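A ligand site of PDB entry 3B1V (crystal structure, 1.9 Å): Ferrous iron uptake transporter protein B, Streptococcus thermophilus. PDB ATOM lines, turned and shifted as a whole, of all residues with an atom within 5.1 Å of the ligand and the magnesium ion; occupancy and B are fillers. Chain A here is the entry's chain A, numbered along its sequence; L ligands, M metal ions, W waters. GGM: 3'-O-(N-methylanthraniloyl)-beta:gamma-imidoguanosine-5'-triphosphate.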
ATOM      1  N   GLY A  10     -17.743 -15.850   5.042  1.00  0.00           N
ATOM      2  CA  GLY A  10     -17.691 -17.249   4.582  1.00  0.00           C
ATOM      3  C   GLY A  10     -18.574 -17.455   3.391  1.00  0.00           C
ATOM      4  O   GLY A  10     -19.376 -16.594   3.069  1.00  0.00           O
ATOM      5  N   ASN A  11     -18.410 -18.610   2.729  1.00  0.00           N
ATOM      6  CA  ASN A  11     -19.166 -18.931   1.529  1.00  0.00           C
ATOM      7  C   ASN A  11     -20.667 -18.908   1.866  1.00  0.00           C
ATOM      8  O   ASN A  11     -21.072 -19.160   2.996  1.00  0.00           O
ATOM      9  CB  ASN A  11     -18.855 -20.343   0.954  1.00  0.00           C
ATOM     10  CG  ASN A  11     -17.384 -20.543   0.499  1.00  0.00           C
ATOM     11  OD1 ASN A  11     -16.993 -21.691   0.207  1.00  0.00           O
ATOM     12  ND2 ASN A  11     -16.581 -19.485   0.438  1.00  0.00           N
ATOM     13  N   PRO A  12     -21.522 -18.632   0.875  1.00  0.00           N
ATOM     14  CA  PRO A  12     -22.947 -18.808   1.190  1.00  0.00           C
ATOM     15  C   PRO A  12     -23.261 -20.256   1.576  1.00  0.00           C
ATOM     16  O   PRO A  12     -22.547 -21.190   1.212  1.00  0.00           O
ATOM     17  CB  PRO A  12     -23.666 -18.396  -0.093  1.00  0.00           C
ATOM     18  CG  PRO A  12     -22.597 -18.266  -1.138  1.00  0.00           C
ATOM     19  CD  PRO A  12     -21.245 -18.244  -0.518  1.00  0.00           C
ATOM     20  N   ASN A  13     -24.330 -20.411   2.344  1.00  0.00           N
ATOM     21  CA  ASN A  13     -24.826 -21.703   2.782  1.00  0.00           C
ATOM     22  C   ASN A  13     -23.805 -22.444   3.668  1.00  0.00           C
ATOM     23  O   ASN A  13     -23.699 -23.674   3.636  1.00  0.00           O
ATOM     24  CB  ASN A  13     -25.236 -22.499   1.520  1.00  0.00           C
ATOM     25  CG  ASN A  13     -26.239 -23.615   1.796  1.00  0.00           C
ATOM     26  OD1 ASN A  13     -26.937 -23.662   2.809  1.00  0.00           O
ATOM     27  ND2 ASN A  13     -26.320 -24.531   0.833  1.00  0.00           N
ATOM     28  N   SER A  14     -23.068 -21.688   4.488  1.00  0.00           N
ATOM     29  CA  SER A  14     -22.098 -22.271   5.435  1.00  0.00           C
ATOM     30  C   SER A  14     -22.529 -22.234   6.904  1.00  0.00           C
ATOM     31  O   SER A  14     -21.867 -22.827   7.780  1.00  0.00           O
ATOM     32  CB  SER A  14     -20.720 -21.627   5.269  1.00  0.00           C
ATOM     33  OG  SER A  14     -20.755 -20.233   5.512  1.00  0.00           O
ATOM     34  N   GLY A  15     -23.669 -21.589   7.187  1.00  0.00           N
ATOM     35  CA  GLY A  15     -24.217 -21.485   8.537  1.00  0.00           C
ATOM     36  C   GLY A  15     -23.932 -20.183   9.258  1.00  0.00           C
ATOM     37  O   GLY A  15     -24.069 -20.113  10.473  1.00  0.00           O
ATOM     38  N   LYS A  16     -23.558 -19.136   8.525  1.00  0.00           N
ATOM     39  CA  LYS A  16     -23.271 -17.850   9.155  1.00  0.00           C
ATOM     40  C   LYS A  16     -24.441 -17.294   9.957  1.00  0.00           C
ATOM     41  O   LYS A  16     -24.273 -16.965  11.137  1.00  0.00           O
ATOM     42  CB  LYS A  16     -22.854 -16.804   8.115  1.00  0.00           C
ATOM     43  CG  LYS A  16     -21.516 -17.127   7.465  1.00  0.00           C
ATOM     44  CD  LYS A  16     -21.056 -16.011   6.470  1.00  0.00           C
ATOM     45  CE  LYS A  16     -21.998 -15.826   5.306  1.00  0.00           C
ATOM     46  NZ  LYS A  16     -22.407 -17.086   4.575  1.00  0.00           N
ATOM     47  N   THR A  17     -25.603 -17.163   9.342  1.00  0.00           N
ATOM     48  CA  THR A  17     -26.778 -16.604  10.015  1.00  0.00           C
ATOM     49  C   THR A  17     -27.274 -17.513  11.163  1.00  0.00           C
ATOM     50  O   THR A  17     -27.729 -17.030  12.221  1.00  0.00           O
ATOM     51  CB  THR A  17     -27.911 -16.222   9.022  1.00  0.00           C
ATOM     52  OG1 THR A  17     -27.421 -15.335   8.001  1.00  0.00           O
ATOM     53  CG2 THR A  17     -29.042 -15.506   9.774  1.00  0.00           C
ATOM     54  N   SER A  18     -27.183 -18.826  10.974  1.00  0.00           N
ATOM     55  CA  SER A  18     -27.515 -19.778  12.029  1.00  0.00           C
ATOM     56  C   SER A  18     -26.668 -19.543  13.277  1.00  0.00           C
ATOM     57  O   SER A  18     -27.189 -19.559  14.391  1.00  0.00           O
ATOM     58  CB  SER A  18     -27.326 -21.230  11.551  1.00  0.00           C
ATOM     59  OG  SER A  18     -28.066 -21.462  10.365  1.00  0.00           O
ATOM     60  N   ARG A  29     -33.144 -14.516   8.870  1.00  0.00           N
ATOM     61  CA  ARG A  29     -33.429 -15.528   7.848  1.00  0.00           C
ATOM     62  C   ARG A  29     -32.313 -16.508   7.604  1.00  0.00           C
ATOM     63  O   ARG A  29     -31.186 -16.124   7.266  1.00  0.00           O
ATOM     64  CB  ARG A  29     -33.807 -14.854   6.537  1.00  0.00           C
ATOM     65  CG  ARG A  29     -35.149 -14.160   6.604  1.00  0.00           C
ATOM     66  CD  ARG A  29     -35.560 -13.609   5.261  1.00  0.00           C
ATOM     67  NE  ARG A  29     -36.887 -13.032   5.334  1.00  0.00           N
ATOM     68  CZ  ARG A  29     -37.575 -12.542   4.300  1.00  0.00           C
ATOM     69  NH1 ARG A  29     -37.048 -12.539   3.082  1.00  0.00           N
ATOM     70  NH2 ARG A  29     -38.787 -12.069   4.497  1.00  0.00           N
ATOM     71  N   VAL A  30     -32.662 -17.780   7.802  1.00  0.00           N
ATOM     72  CA  VAL A  30     -31.843 -18.959   7.550  1.00  0.00           C
ATOM     73  C   VAL A  30     -32.565 -19.824   6.523  1.00  0.00           C
ATOM     74  O   VAL A  30     -33.787 -20.032   6.631  1.00  0.00           O
ATOM     75  CB  VAL A  30     -31.623 -19.762   8.844  1.00  0.00           C
ATOM     76  CG1 VAL A  30     -30.964 -21.120   8.554  1.00  0.00           C
ATOM     77  CG2 VAL A  30     -30.797 -18.933   9.834  1.00  0.00           C
ATOM     78  N   GLY A  31     -31.832 -20.333   5.539  1.00  0.00           N
ATOM     79  CA  GLY A  31     -32.419 -21.108   4.437  1.00  0.00           C
ATOM     80  C   GLY A  31     -31.450 -22.124   3.858  1.00  0.00           C
ATOM     81  O   GLY A  31     -30.242 -21.952   3.996  1.00  0.00           O
ATOM     82  N   ASN A  32     -31.969 -23.162   3.212  1.00  0.00           N
ATOM     83  CA  ASN A  32     -31.143 -24.275   2.704  1.00  0.00           C
ATOM     84  C   ASN A  32     -30.603 -24.084   1.281  1.00  0.00           C
ATOM     85  O   ASN A  32     -30.428 -25.047   0.566  1.00  0.00           O
ATOM     86  CB  ASN A  32     -31.863 -25.636   2.852  1.00  0.00           C
ATOM     87  CG  ASN A  32     -32.992 -25.822   1.838  1.00  0.00           C
ATOM     88  OD1 ASN A  32     -33.460 -24.845   1.295  1.00  0.00           O
ATOM     89  ND2 ASN A  32     -33.417 -27.060   1.591  1.00  0.00           N
ATOM     90  N   TRP A  33     -30.326 -22.846   0.877  1.00  0.00           N
ATOM     91  CA  TRP A  33     -29.739 -22.576  -0.431  1.00  0.00           C
ATOM     92  C   TRP A  33     -28.780 -21.394  -0.288  1.00  0.00           C
ATOM     93  O   TRP A  33     -28.896 -20.602   0.660  1.00  0.00           O
ATOM     94  CB  TRP A  33     -30.810 -22.296  -1.490  1.00  0.00           C
ATOM     95  CG  TRP A  33     -31.549 -20.989  -1.304  1.00  0.00           C
ATOM     96  CD1 TRP A  33     -31.265 -19.773  -1.910  1.00  0.00           C
ATOM     97  CD2 TRP A  33     -32.659 -20.740  -0.442  1.00  0.00           C
ATOM     98  NE1 TRP A  33     -32.151 -18.811  -1.469  1.00  0.00           N
ATOM     99  CE2 TRP A  33     -33.012 -19.373  -0.566  1.00  0.00           C
ATOM    100  CE3 TRP A  33     -33.401 -21.547   0.437  1.00  0.00           C
ATOM    101  CZ2 TRP A  33     -34.068 -18.811   0.152  1.00  0.00           C
ATOM    102  CZ3 TRP A  33     -34.465 -20.984   1.144  1.00  0.00           C
ATOM    103  CH2 TRP A  33     -34.784 -19.629   0.984  1.00  0.00           C
ATOM    104  N   PRO A  34     -27.811 -21.283  -1.206  1.00  0.00           N
ATOM    105  CA  PRO A  34     -26.869 -20.157  -1.117  1.00  0.00           C
ATOM    106  C   PRO A  34     -27.509 -18.851  -1.563  1.00  0.00           C
ATOM    107  O   PRO A  34     -28.167 -18.811  -2.590  1.00  0.00           O
ATOM    108  CB  PRO A  34     -25.759 -20.558  -2.108  1.00  0.00           C
ATOM    109  CG  PRO A  34     -26.390 -21.486  -3.050  1.00  0.00           C
ATOM    110  CD  PRO A  34     -27.486 -22.200  -2.313  1.00  0.00           C
ATOM    111  N   GLY A  35     -27.278 -17.788  -0.797  1.00  0.00           N
ATOM    112  CA  GLY A  35     -27.748 -16.448  -1.137  1.00  0.00           C
ATOM    113  C   GLY A  35     -28.977 -16.020  -0.364  1.00  0.00           C
ATOM    114  O   GLY A  35     -29.804 -15.284  -0.882  1.00  0.00           O
ATOM    115  N   VAL A  36     -29.108 -16.456   0.881  1.00  0.00           N
ATOM    116  CA  VAL A  36     -30.234 -16.045   1.725  1.00  0.00           C
ATOM    117  C   VAL A  36     -30.033 -14.646   2.262  1.00  0.00           C
ATOM    118  O   VAL A  36     -30.897 -13.780   2.066  1.00  0.00           O
ATOM    119  CB  VAL A  36     -30.473 -17.034   2.850  1.00  0.00           C
ATOM    120  CG1 VAL A  36     -31.514 -16.479   3.866  1.00  0.00           C
ATOM    121  CG2 VAL A  36     -30.938 -18.383   2.277  1.00  0.00           C
ATOM    122  N   THR A  37     -28.910 -14.393   2.950  1.00  0.00           N
ATOM    123  CA  THR A  37     -28.660 -13.062   3.505  1.00  0.00           C
ATOM    124  C   THR A  37     -28.203 -12.109   2.401  1.00  0.00           C
ATOM    125  O   THR A  37     -27.340 -12.468   1.624  1.00  0.00           O
ATOM    126  CB  THR A  37     -27.571 -13.125   4.624  1.00  0.00           C
ATOM    127  OG1 THR A  37     -28.000 -14.046   5.622  1.00  0.00           O
ATOM    128  CG2 THR A  37     -27.318 -11.739   5.235  1.00  0.00           C
ATOM    129  N   ASP A  55     -23.486 -10.031  10.724  1.00  0.00           N
ATOM    130  CA  ASP A  55     -23.861 -11.042   9.743  1.00  0.00           C
ATOM    131  C   ASP A  55     -23.798 -10.357   8.395  1.00  0.00           C
ATOM    132  O   ASP A  55     -24.164  -9.181   8.236  1.00  0.00           O
ATOM    133  CB  ASP A  55     -25.291 -11.556   9.986  1.00  0.00           C
ATOM    134  CG  ASP A  55     -25.635 -12.789   9.148  1.00  0.00           C
ATOM    135  OD1 ASP A  55     -24.695 -13.476   8.656  1.00  0.00           O
ATOM    136  OD2 ASP A  55     -26.859 -13.089   8.982  1.00  0.00           O
ATOM    137  N   LEU A  56     -23.300 -11.086   7.406  1.00  0.00           N
ATOM    138  CA  LEU A  56     -23.063 -10.508   6.104  1.00  0.00           C
ATOM    139  C   LEU A  56     -23.398 -11.539   5.047  1.00  0.00           C
ATOM    140  O   LEU A  56     -23.382 -12.752   5.322  1.00  0.00           O
ATOM    141  CB  LEU A  56     -21.590 -10.086   5.988  1.00  0.00           C
ATOM    142  CG  LEU A  56     -21.158  -8.847   6.779  1.00  0.00           C
ATOM    143  CD1 LEU A  56     -19.683  -8.883   7.142  1.00  0.00           C
ATOM    144  CD2 LEU A  56     -21.519  -7.575   6.015  1.00  0.00           C
ATOM    145  N   PRO A  57     -23.703 -11.074   3.821  1.00  0.00           N
ATOM    146  CA  PRO A  57     -23.913 -12.019   2.731  1.00  0.00           C
ATOM    147  C   PRO A  57     -22.700 -12.923   2.511  1.00  0.00           C
ATOM    148  O   PRO A  57     -21.537 -12.530   2.731  1.00  0.00           O
ATOM    149  CB  PRO A  57     -24.100 -11.105   1.529  1.00  0.00           C
ATOM    150  CG  PRO A  57     -24.605  -9.813   2.106  1.00  0.00           C
ATOM    151  CD  PRO A  57     -23.778  -9.679   3.341  1.00  0.00           C
ATOM    152  N   GLY A  58     -22.979 -14.147   2.076  1.00  0.00           N
ATOM    153  CA  GLY A  58     -21.938 -15.065   1.682  1.00  0.00           C
ATOM    154  C   GLY A  58     -21.099 -14.603   0.503  1.00  0.00           C
ATOM    155  O   GLY A  58     -21.525 -13.814  -0.336  1.00  0.00           O
ATOM    156  N   ASN A 115     -17.599 -25.188  10.798  1.00  0.00           N
ATOM    157  CA  ASN A 115     -19.013 -25.428  11.029  1.00  0.00           C
ATOM    158  C   ASN A 115     -19.520 -26.670  10.284  1.00  0.00           C
ATOM    159  O   ASN A 115     -18.808 -27.255   9.476  1.00  0.00           O
ATOM    160  CB  ASN A 115     -19.823 -24.177  10.660  1.00  0.00           C
ATOM    161  CG  ASN A 115     -21.203 -24.164  11.278  1.00  0.00           C
ATOM    162  OD1 ASN A 115     -21.394 -24.558  12.421  1.00  0.00           O
ATOM    163  ND2 ASN A 115     -22.198 -23.717  10.505  1.00  0.00           N
ATOM    164  N   MET A 116     -20.744 -27.084  10.604  1.00  0.00           N
ATOM    165  CA  MET A 116     -21.318 -28.327  10.069  1.00  0.00           C
ATOM    166  C   MET A 116     -20.464 -29.541  10.435  1.00  0.00           C
ATOM    167  O   MET A 116     -20.390 -30.519   9.688  1.00  0.00           O
ATOM    168  CB  MET A 116     -21.530 -28.211   8.556  1.00  0.00           C
ATOM    169  CG  MET A 116     -22.440 -27.044   8.202  1.00  0.00           C
ATOM    170  SD  MET A 116     -22.668 -26.807   6.437  1.00  0.00           S
ATOM    171  CE  MET A 116     -24.063 -25.654   6.498  1.00  0.00           C
ATOM    172  N   ILE A 117     -19.812 -29.482  11.581  1.00  0.00           N
ATOM    173  CA  ILE A 117     -18.958 -30.587  12.001  1.00  0.00           C
ATOM    174  C   ILE A 117     -19.809 -31.846  12.248  1.00  0.00           C
ATOM    175  O   ILE A 117     -19.318 -32.966  12.149  1.00  0.00           O
ATOM    176  CB  ILE A 117     -18.136 -30.230  13.279  1.00  0.00           C
ATOM    177  CG1 ILE A 117     -16.845 -31.058  13.352  1.00  0.00           C
ATOM    178  CG2 ILE A 117     -19.002 -30.370  14.552  1.00  0.00           C
ATOM    179  CD1 ILE A 117     -15.800 -30.659  12.315  1.00  0.00           C
ATOM    180  N   ASP A 118     -21.100 -31.636  12.560  1.00  0.00           N
ATOM    181  CA  ASP A 118     -22.029 -32.761  12.762  1.00  0.00           C
ATOM    182  C   ASP A 118     -22.318 -33.569  11.470  1.00  0.00           C
ATOM    183  O   ASP A 118     -22.598 -34.766  11.534  1.00  0.00           O
ATOM    184  CB  ASP A 118     -23.348 -32.277  13.369  1.00  0.00           C
ATOM    185  CG  ASP A 118     -24.043 -31.254  12.495  1.00  0.00           C
ATOM    186  OD1 ASP A 118     -23.529 -30.105  12.375  1.00  0.00           O
ATOM    187  OD2 ASP A 118     -25.090 -31.591  11.920  1.00  0.00           O
ATOM    188  N   VAL A 119     -22.268 -32.904  10.325  1.00  0.00           N
ATOM    189  CA  VAL A 119     -22.439 -33.562   9.037  1.00  0.00           C
ATOM    190  C   VAL A 119     -21.191 -34.378   8.737  1.00  0.00           C
ATOM    191  O   VAL A 119     -21.275 -35.516   8.235  1.00  0.00           O
ATOM    192  CB  VAL A 119     -22.658 -32.558   7.894  1.00  0.00           C
ATOM    193  CG1 VAL A 119     -22.883 -33.295   6.569  1.00  0.00           C
ATOM    194  CG2 VAL A 119     -23.817 -31.618   8.211  1.00  0.00           C
ATOM    195  N   THR A 143     -17.487 -26.282  15.174  1.00  0.00           N
ATOM    196  CA  THR A 143     -18.806 -25.842  15.618  1.00  0.00           C
ATOM    197  C   THR A 143     -19.940 -26.547  14.887  1.00  0.00           C
ATOM    198  O   THR A 143     -19.765 -27.069  13.778  1.00  0.00           O
ATOM    199  CB  THR A 143     -19.010 -24.308  15.406  1.00  0.00           C
ATOM    200  OG1 THR A 143     -19.033 -24.019  14.007  1.00  0.00           O
ATOM    201  CG2 THR A 143     -17.911 -23.480  16.068  1.00  0.00           C
ATOM    202  N   SER A 144     -21.094 -26.571  15.536  1.00  0.00           N
ATOM    203  CA  SER A 144     -22.329 -26.991  14.880  1.00  0.00           C
ATOM    204  C   SER A 144     -23.439 -26.078  15.361  1.00  0.00           C
ATOM    205  O   SER A 144     -23.747 -26.035  16.552  1.00  0.00           O
ATOM    206  CB  SER A 144     -22.684 -28.444  15.199  1.00  0.00           C
ATOM    207  OG  SER A 144     -23.965 -28.743  14.669  1.00  0.00           O
ATOM    208  N   ALA A 145     -24.034 -25.331  14.423  1.00  0.00           N
ATOM    209  CA  ALA A 145     -25.191 -24.492  14.737  1.00  0.00           C
ATOM    210  C   ALA A 145     -26.416 -25.368  15.015  1.00  0.00           C
ATOM    211  O   ALA A 145     -27.284 -24.949  15.783  1.00  0.00           O
ATOM    212  CB  ALA A 145     -25.460 -23.509  13.629  1.00  0.00           C
ATOM    213  N   LEU A 146     -26.475 -26.550  14.401  1.00  0.00           N
ATOM    214  CA  LEU A 146     -27.557 -27.497  14.611  1.00  0.00           C
ATOM    215  C   LEU A 146     -27.537 -28.087  16.021  1.00  0.00           C
ATOM    216  O   LEU A 146     -28.537 -28.048  16.737  1.00  0.00           O
ATOM    217  CB  LEU A 146     -27.477 -28.653  13.603  1.00  0.00           C
ATOM    218  CG  LEU A 146     -28.612 -29.695  13.684  1.00  0.00           C
ATOM    219  CD1 LEU A 146     -29.977 -29.042  13.508  1.00  0.00           C
ATOM    220  CD2 LEU A 146     -28.420 -30.803  12.650  1.00  0.00           C
HETATM  221  N1  GGM L   1     -24.976 -28.314  10.833  1.00  0.00           N
HETATM  222  C2  GGM L   1     -25.989 -28.625   9.907  1.00  0.00           C
HETATM  223  N2  GGM L   1     -26.314 -29.900   9.652  1.00  0.00           N
HETATM  224  N3  GGM L   1     -26.608 -27.618   9.275  1.00  0.00           N
HETATM  225  C4  GGM L   1     -26.273 -26.329   9.498  1.00  0.00           C
HETATM  226  C5  GGM L   1     -25.301 -25.961  10.407  1.00  0.00           C
HETATM  227  C6  GGM L   1     -24.635 -26.970  11.082  1.00  0.00           C
HETATM  228  O6  GGM L   1     -23.757 -26.692  11.894  1.00  0.00           O
HETATM  229  N7  GGM L   1     -25.228 -24.618  10.405  1.00  0.00           N
HETATM  230  C8  GGM L   1     -26.120 -24.147   9.539  1.00  0.00           C
HETATM  231  N9  GGM L   1     -26.766 -25.191   8.997  1.00  0.00           N
HETATM  232  PA  GGM L   1     -27.494 -20.294   6.892  1.00  0.00           P
HETATM  233  PB  GGM L   1     -25.459 -18.681   5.553  1.00  0.00           P
HETATM  234  PG  GGM L   1     -25.925 -17.012   3.185  1.00  0.00           P
HETATM  235  C1' GGM L   1     -27.798 -25.264   8.000  1.00  0.00           C
HETATM  236  O1A GGM L   1     -27.328 -19.918   8.299  1.00  0.00           O
HETATM  237  O1B GGM L   1     -23.962 -18.908   5.563  1.00  0.00           O
HETATM  238  O1G GGM L   1     -26.800 -16.094   3.960  1.00  0.00           O
HETATM  239  C2' GGM L   1     -28.988 -24.409   7.986  1.00  0.00           C
HETATM  240  O2' GGM L   1     -30.034 -24.965   8.860  1.00  0.00           O
HETATM  241  O2A GGM L   1     -28.612 -19.672   6.130  1.00  0.00           O
HETATM  242  O2B GGM L   1     -25.986 -17.579   6.393  1.00  0.00           O
HETATM  243  O2G GGM L   1     -24.377 -16.513   3.100  1.00  0.00           O
HETATM  244  C3' GGM L   1     -29.571 -23.872   6.780  1.00  0.00           C
HETATM  245  O3' GGM L   1     -30.483 -24.914   6.314  1.00  0.00           O
HETATM  246  O3A GGM L   1     -26.093 -20.090   5.995  1.00  0.00           O
HETATM  247  N3B GGM L   1     -26.021 -18.496   3.989  1.00  0.00           N
HETATM  248  O3G GGM L   1     -26.490 -17.168   1.708  1.00  0.00           O
HETATM  249  C4' GGM L   1     -28.230 -23.975   5.963  1.00  0.00           C
HETATM  250  O4' GGM L   1     -27.247 -24.828   6.698  1.00  0.00           O
HETATM  251  C5' GGM L   1     -27.505 -22.654   5.727  1.00  0.00           C
HETATM  252  O5' GGM L   1     -27.564 -21.858   6.898  1.00  0.00           O
HETATM  253 MG    MG M   1     -27.009 -15.865   5.935  1.00  0.00          MG
HETATM  254  O   HOH W   1     -28.865 -16.995   6.007  1.00  0.00           O
HETATM  255  O   HOH W   2     -33.064 -24.223   6.236  1.00  0.00           O
HETATM  256  O   HOH W   3     -25.859 -14.612   0.859  1.00  0.00           O
HETATM  257  O   HOH W   4     -25.197 -14.682   6.255  1.00  0.00           O
HETATM  258  O   HOH W   5     -28.115 -20.172   3.188  1.00  0.00           O
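Water W4 lies within hydrogen-bond range of OD1 of Asp 55 and O of Leu 56. Water W1 bridges O2A of the ligand (2.7 Å) and O of Arg 29 (2.8 Å). Water W2 bridges O3' of the ligand (2.7 Å) and N of Asn 32 (3.4 Å). Water W3 lies within hydrogen-bond range of O of Thr 37 (2.7 Å), O3G of the ligand (2.8 Å) and N of Gly 58 (3.2 Å). Water W5 lies within hydrogen-bond range of the backbone carbonyl oxygen of Trp 33, a nitrogen (N3B) of the ligand and the backbone carbonyl oxygen of Gly 31.
N of Asn 13 lies close to N3B of the ligand (3.0 Å). Residues that only touch the ligand: Asn 11, Pro 12, Val 30, Asn 32, Pro 34, Val 119 and Leu 146. Hydrophobic or aromatic side chains within 4 Å of the ligand: Pro 12, Val 30, Val 36, Met 116, Val 119, Ala 145 and Leu 146.
An oxygen (O1G) of the ligand lies close to the backbone NH (N) of Thr 37 (2.9 Å). The backbone NH (N) of Thr 17 is in hydrogen-bond range of an oxygen (O1A) of the ligand, at 3.4 Å. The backbone NH (N) of Lys 16 lies within hydrogen-bond range of an oxygen (O1B) of the ligand, at 3.0 Å. The side-chain amino group (NZ) of Lys 16 is in salt-bridge range of an oxygen (O2G) of the ligand, 2.5 Å away. The backbone NH of Ser 18 sits at hydrogen-bond distance from an oxygen (O1A) of the ligand (2.9 Å). O1A of the ligand lies within hydrogen-bond range of OG of Ser 18 (2.7 Å). The backbone NH (N) of Gly 35 is in hydrogen-bond range of an oxygen (O3G) of the ligand, at 2.7 Å. A nitrogen (N1) of the ligand lies within hydrogen-bond range of the side-chain carboxylate (OD1) of Asp 118 (2.8 Å). N of Val 36 is in hydrogen-bond range of O3G of the ligand (2.8 Å). O6 of the ligand sits at hydrogen-bond distance from N of Ala 145 (2.9 Å). O2G of the ligand sits at hydrogen-bond distance from N of Gly 58, 2.9 Å away. N of Gly 15 is in hydrogen-bond range of O3A of the ligand (3.1 Å). The backbone NH of Ser 14 is in hydrogen-bond range of an oxygen (O1B) of the ligand, 3.1 Å away. The side-chain hydroxyl (OG) of Ser 14 sits at hydrogen-bond distance from an oxygen (O1B) of the ligand, at 3.5 Å. N7 of the ligand lies within hydrogen-bond range of ND2 of Asn 115 (3.2 Å). An oxygen (O6) of the ligand lies within hydrogen-bond range of the backbone NH of Met 116 (3.3 Å). An oxygen (O2A) of the ligand lies within hydrogen-bond range of the backbone NH of Gly 31 (3.3 Å). The side-chain hydroxyl (OG) of Ser 144 lies close to an oxygen (O6) of the ligand (3.5 Å).
O1G of the ligand binds the magnesium ion (2.0 Å). The magnesium ion is bound by O2B of the ligand (2.0 Å). OG1 of Thr 37 binds the magnesium ion (2.1 Å). OG1 of Thr 17 binds the magnesium ion (2.2 Å). Water W1 binds the magnesium ion, 2.2 Å away. Water W4 binds the magnesium ion (2.2 Å).
Of the 31 residues printed, 2 come within 4 Å of the magnesium ion.
OD2 of Asp 55 lies close to OG1 of Thr 17 (2.5 Å). The backbone carbonyl oxygen (O) of Asn 11 lies within hydrogen-bond range of the side-chain amino group (NZ) of Lys 16. The side-chain carboxylate of Asp 118 lies within hydrogen-bond range of the side-chain hydroxyl of Ser 144 (2.7 Å). OD1 of Asn 115 sits at hydrogen-bond distance from N of Ala 145, at 3.4 Å. OG of Ser 14 is in hydrogen-bond range of O of Asn 11, 2.8 Å away. The side-chain hydroxyl (OG1) of Thr 143 is in hydrogen-bond range of the side-chain amide oxygen (OD1) of Asn 115 (2.9 Å). The backbone NH (N) of Met 116 sits at hydrogen-bond distance from the backbone carbonyl oxygen (O) of Thr 143. The backbone NH (N) of Leu 146 lies close to the side-chain hydroxyl (OG) of Ser 144, 3.3 Å away.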
